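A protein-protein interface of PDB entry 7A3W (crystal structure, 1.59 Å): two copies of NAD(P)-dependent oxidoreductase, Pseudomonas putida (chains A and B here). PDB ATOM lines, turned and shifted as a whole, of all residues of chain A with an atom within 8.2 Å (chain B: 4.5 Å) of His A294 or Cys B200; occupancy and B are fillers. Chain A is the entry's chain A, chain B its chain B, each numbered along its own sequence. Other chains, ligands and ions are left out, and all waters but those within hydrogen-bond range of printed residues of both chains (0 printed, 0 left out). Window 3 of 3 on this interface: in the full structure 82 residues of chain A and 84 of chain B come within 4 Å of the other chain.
O of Val B196 sits at hydrogen-bond distance from SG of Cys B200, 3.4 Å away.
The side-chain sulfur of Cys B200 is in hydrogen-bond range of the backbone carbonyl oxygen of Ala B259, at 3.7 Å.
Among the printed residues, merely in contact across the chains: Pro A175 with Ala B201 (3.5 Å), Ala A179 with Leu B197 (3.8 Å), Ala A179 with Ala B198 (3.9 Å) and Phe A290 with Val B196 (3.8 Å).
No position is printed for both chains.
Of the 6 pairs that touch across the chains among the printed residues, none has its exchanged pair printed and touching as well.
A ring nitrogen (ND1) of His A294 lies close to the side-chain hydroxyl (OG) of Ser B199 (3.5 Å).
The side-chain sulfur (SG) of Cys B200 is in hydrogen-bond range of a ring nitrogen (NE2) of His A294, 3.6 Å away.
Printed residues of chain B within 4 Å of His A294: Ser B199 and Cys B200.
Cys B200 touches just one residue of chain A: His A294 (3.6 Å).
Ser B199 touches just one residue of chain A: His A294 (3.1 Å).
Of the printed residues of chain A, Ala B198 touches Ala A179.
Printed residues of chain B within 4 Å of Ala A179: Leu B197 and Ala B198.
Of the printed residues of chain A, Val B196 touches Phe A290.
Of the printed residues of chain B, Pro A175 touches Ala B201 (3.5 Å).
The nearest printed residue of chain B that does not touch His A294 is Val B196 (4.01 Å).
The nearest residue of chain A that does not touch Cys B200 is Pro A175 (6.7 Å).
Printed residues of chain B that touch a printed residue of chain A: Val B196, Leu B197, Ala B198, Ser B199, Cys B200 and Ala B201.
Hydrophobic or aromatic side chains of chain B that line the printed part of chain A: Val B196, Leu B197 and Ala B201.
Printed residues of chain A that touch a printed residue of chain B: Pro A175, Ala A179, Phe A290 and His A294.
Hydrophobic or aromatic side chains of chain A within 4 Å of the printed part of chain B: Pro A175, Ala A179, Phe A290 and His A294.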
ATOM      1  N   PRO A 175       5.342   6.241 -18.958  1.00  0.00           N
ATOM      2  CA  PRO A 175       4.782   4.905 -19.159  1.00  0.00           C
ATOM      3  C   PRO A 175       5.403   3.849 -18.243  1.00  0.00           C
ATOM      4  O   PRO A 175       4.684   3.006 -17.732  1.00  0.00           O
ATOM      5  CB  PRO A 175       5.017   4.630 -20.643  1.00  0.00           C
ATOM      6  CG  PRO A 175       5.146   6.018 -21.256  1.00  0.00           C
ATOM      7  CD  PRO A 175       5.896   6.800 -20.202  1.00  0.00           C
ATOM      8  N   ALA A 179       3.434   1.848 -15.397  1.00  0.00           N
ATOM      9  CA  ALA A 179       3.483   0.370 -15.507  1.00  0.00           C
ATOM     10  C   ALA A 179       3.938  -0.231 -14.176  1.00  0.00           C
ATOM     11  O   ALA A 179       3.330  -1.230 -13.706  1.00  0.00           O
ATOM     12  CB  ALA A 179       4.377  -0.094 -16.638  1.00  0.00           C
ATOM     13  N   ILE A 230       8.770 -15.273 -21.415  1.00  0.00           N
ATOM     14  CA  ILE A 230       8.111 -14.335 -22.364  1.00  0.00           C
ATOM     15  C   ILE A 230       9.158 -13.869 -23.392  1.00  0.00           C
ATOM     16  O   ILE A 230       8.838 -13.855 -24.590  1.00  0.00           O
ATOM     17  CB  ILE A 230       7.427 -13.179 -21.609  1.00  0.00           C
ATOM     18  CG1 ILE A 230       6.266 -13.698 -20.743  1.00  0.00           C
ATOM     19  CG2 ILE A 230       6.970 -12.106 -22.581  1.00  0.00           C
ATOM     20  CD1 ILE A 230       5.838 -12.784 -19.617  1.00  0.00           C
ATOM     21  N   MET A 275      -9.038 -16.167 -20.485  1.00  0.00           N
ATOM     22  CA  MET A 275      -8.550 -15.659 -21.788  1.00  0.00           C
ATOM     23  C   MET A 275      -7.577 -16.659 -22.398  1.00  0.00           C
ATOM     24  O   MET A 275      -7.761 -17.002 -23.577  1.00  0.00           O
ATOM     25  CB  MET A 275      -7.812 -14.332 -21.638  1.00  0.00           C
ATOM     26  CG  MET A 275      -8.575 -13.164 -22.186  1.00  0.00           C
ATOM     27  SD  MET A 275      -7.646 -11.654 -21.843  1.00  0.00           S
ATOM     28  CE  MET A 275      -8.695 -10.919 -20.593  1.00  0.00           C
ATOM     29  N   SER A 288       2.229 -17.716 -20.189  1.00  0.00           N
ATOM     30  CA  SER A 288       1.487 -17.602 -21.475  1.00  0.00           C
ATOM     31  C   SER A 288       0.353 -16.567 -21.362  1.00  0.00           C
ATOM     32  O   SER A 288      -0.173 -16.149 -22.400  1.00  0.00           O
ATOM     33  CB  SER A 288       0.946 -18.934 -21.923  1.00  0.00           C
ATOM     34  OG  SER A 288      -0.066 -19.404 -21.044  1.00  0.00           O
ATOM     35  N   LEU A 289      -0.069 -16.210 -20.156  1.00  0.00           N
ATOM     36  CA  LEU A 289      -1.102 -15.152 -19.971  1.00  0.00           C
ATOM     37  C   LEU A 289      -0.655 -13.849 -20.656  1.00  0.00           C
ATOM     38  O   LEU A 289      -1.504 -13.142 -21.182  1.00  0.00           O
ATOM     39  CB  LEU A 289      -1.339 -14.921 -18.479  1.00  0.00           C
ATOM     40  CG  LEU A 289      -2.528 -15.678 -17.890  1.00  0.00           C
ATOM     41  CD1 LEU A 289      -2.439 -17.182 -18.134  1.00  0.00           C
ATOM     42  CD2 LEU A 289      -2.608 -15.384 -16.414  1.00  0.00           C
ATOM     43  N   PHE A 290       0.641 -13.563 -20.672  1.00  0.00           N
ATOM     44  CA  PHE A 290       1.200 -12.350 -21.318  1.00  0.00           C
ATOM     45  C   PHE A 290       0.780 -12.331 -22.785  1.00  0.00           C
ATOM     46  O   PHE A 290       0.364 -11.273 -23.259  1.00  0.00           O
ATOM     47  CB  PHE A 290       2.718 -12.332 -21.216  1.00  0.00           C
ATOM     48  CG  PHE A 290       3.344 -11.103 -21.818  1.00  0.00           C
ATOM     49  CD1 PHE A 290       3.700 -11.083 -23.151  1.00  0.00           C
ATOM     50  CD2 PHE A 290       3.626  -9.992 -21.037  1.00  0.00           C
ATOM     51  CE1 PHE A 290       4.312  -9.962 -23.696  1.00  0.00           C
ATOM     52  CE2 PHE A 290       4.222  -8.870 -21.589  1.00  0.00           C
ATOM     53  CZ  PHE A 290       4.575  -8.860 -22.920  1.00  0.00           C
ATOM     54  N   LYS A 291       0.903 -13.471 -23.466  1.00  0.00           N
ATOM     55  CA  LYS A 291       0.595 -13.594 -24.914  1.00  0.00           C
ATOM     56  C   LYS A 291      -0.924 -13.457 -25.076  1.00  0.00           C
ATOM     57  O   LYS A 291      -1.341 -12.804 -26.035  1.00  0.00           O
ATOM     58  CB  LYS A 291       1.190 -14.885 -25.494  1.00  0.00           C
ATOM     59  CG  LYS A 291       1.726 -14.790 -26.923  1.00  0.00           C
ATOM     60  N   ALA A 292      -1.735 -14.012 -24.164  1.00  0.00           N
ATOM     61  CA  ALA A 292      -3.217 -13.927 -24.207  1.00  0.00           C
ATOM     62  C   ALA A 292      -3.672 -12.481 -23.996  1.00  0.00           C
ATOM     63  O   ALA A 292      -4.666 -12.046 -24.620  1.00  0.00           O
ATOM     64  CB  ALA A 292      -3.834 -14.845 -23.168  1.00  0.00           C
ATOM     65  N   MET A 293      -2.949 -11.752 -23.149  1.00  0.00           N
ATOM     66  CA  MET A 293      -3.259 -10.361 -22.733  1.00  0.00           C
ATOM     67  C   MET A 293      -2.783  -9.340 -23.758  1.00  0.00           C
ATOM     68  O   MET A 293      -3.463  -8.298 -23.932  1.00  0.00           O
ATOM     69  CB  MET A 293      -2.568 -10.065 -21.400  1.00  0.00           C
ATOM     70  CG  MET A 293      -3.246 -10.740 -20.227  1.00  0.00           C
ATOM     71  SD  MET A 293      -2.153 -10.712 -18.787  1.00  0.00           S
ATOM     72  CE  MET A 293      -2.408  -9.016 -18.278  1.00  0.00           C
ATOM     73  N   HIS A 294      -1.608  -9.537 -24.342  1.00  0.00           N
ATOM     74  CA  HIS A 294      -1.022  -8.459 -25.170  1.00  0.00           C
ATOM     75  C   HIS A 294      -1.557  -8.577 -26.607  1.00  0.00           C
ATOM     76  O   HIS A 294      -1.718  -9.622 -27.274  1.00  0.00           O
ATOM     77  CB  HIS A 294       0.499  -8.406 -24.971  1.00  0.00           C
ATOM     78  CG  HIS A 294       1.102  -7.236 -25.658  1.00  0.00           C
ATOM     79  ND1 HIS A 294       2.466  -7.072 -25.788  1.00  0.00           N
ATOM     80  CD2 HIS A 294       0.514  -6.169 -26.249  1.00  0.00           C
ATOM     81  CE1 HIS A 294       2.705  -5.964 -26.462  1.00  0.00           C
ATOM     82  NE2 HIS A 294       1.517  -5.393 -26.765  1.00  0.00           N
ATOM     83  N   VAL B 196       2.752  -5.664 -19.695  1.00  0.00           N
ATOM     84  CA  VAL B 196       2.059  -5.413 -20.986  1.00  0.00           C
ATOM     85  C   VAL B 196       2.059  -3.906 -21.265  1.00  0.00           C
ATOM     86  O   VAL B 196       2.445  -3.516 -22.392  1.00  0.00           O
ATOM     87  CB  VAL B 196       0.664  -6.043 -21.019  1.00  0.00           C
ATOM     88  CG1 VAL B 196      -0.143  -5.512 -22.188  1.00  0.00           C
ATOM     89  CG2 VAL B 196       0.747  -7.559 -21.063  1.00  0.00           C
ATOM     90  N   LEU B 197       1.700  -3.073 -20.287  1.00  0.00           N
ATOM     91  CA  LEU B 197       1.751  -1.598 -20.483  1.00  0.00           C
ATOM     92  C   LEU B 197       3.170  -1.193 -20.888  1.00  0.00           C
ATOM     93  O   LEU B 197       3.335  -0.428 -21.863  1.00  0.00           O
ATOM     94  CB  LEU B 197       1.292  -0.879 -19.210  1.00  0.00           C
ATOM     95  CG  LEU B 197       1.187   0.652 -19.321  1.00  0.00           C
ATOM     96  CD1 LEU B 197       0.238   1.053 -20.441  1.00  0.00           C
ATOM     97  CD2 LEU B 197       0.698   1.261 -18.016  1.00  0.00           C
ATOM     98  N   ALA B 198       4.190  -1.682 -20.194  1.00  0.00           N
ATOM     99  CA  ALA B 198       5.590  -1.290 -20.485  1.00  0.00           C
ATOM    100  C   ALA B 198       5.936  -1.657 -21.931  1.00  0.00           C
ATOM    101  O   ALA B 198       6.478  -0.821 -22.675  1.00  0.00           O
ATOM    102  CB  ALA B 198       6.518  -1.963 -19.533  1.00  0.00           C
ATOM    103  N   SER B 199       5.592  -2.884 -22.317  1.00  0.00           N
ATOM    104  CA  SER B 199       5.827  -3.430 -23.666  1.00  0.00           C
ATOM    105  C   SER B 199       5.165  -2.525 -24.711  1.00  0.00           C
ATOM    106  O   SER B 199       5.826  -2.259 -25.741  1.00  0.00           O
ATOM    107  CB  SER B 199       5.346  -4.859 -23.762  1.00  0.00           C
ATOM    108  OG  SER B 199       5.405  -5.307 -25.100  1.00  0.00           O
ATOM    109  N   CYS B 200       3.930  -2.057 -24.466  1.00  0.00           N
ATOM    110  CA  CYS B 200       3.186  -1.162 -25.384  1.00  0.00           C
ATOM    111  C   CYS B 200       3.939   0.166 -25.563  1.00  0.00           C
ATOM    112  O   CYS B 200       3.754   0.816 -26.607  1.00  0.00           O
ATOM    113  CB  CYS B 200       1.764  -0.892 -24.922  1.00  0.00           C
ATOM    114  SG  CYS B 200       0.663  -2.335 -24.987  1.00  0.00           S
ATOM    115  N   ALA B 201       4.814   0.529 -24.621  1.00  0.00           N
ATOM    116  CA  ALA B 201       5.603   1.772 -24.658  1.00  0.00           C
ATOM    117  C   ALA B 201       7.034   1.470 -25.120  1.00  0.00           C
ATOM    118  O   ALA B 201       7.867   2.385 -25.068  1.00  0.00           O
ATOM    119  CB  ALA B 201       5.579   2.404 -23.287  1.00  0.00           C
ATOM    120  N   GLY B 202       7.296   0.252 -25.591  1.00  0.00           N
ATOM    121  CA  GLY B 202       8.580  -0.151 -26.188  1.00  0.00           C
ATOM    122  C   GLY B 202       9.583  -0.548 -25.140  1.00  0.00           C
ATOM    123  O   GLY B 202      10.774  -0.676 -25.486  1.00  0.00           O
ATOM    124  N   ALA B 259      -3.239   2.363 -24.275  1.00  0.00           N
ATOM    125  CA  ALA B 259      -2.367   1.278 -24.791  1.00  0.00           C
ATOM    126  C   ALA B 259      -3.202   0.087 -25.271  1.00  0.00           C
ATOM    127  O   ALA B 259      -2.607  -0.867 -25.795  1.00  0.00           O
ATOM    128  CB  ALA B 259      -1.396   0.828 -23.730  1.00  0.00           C
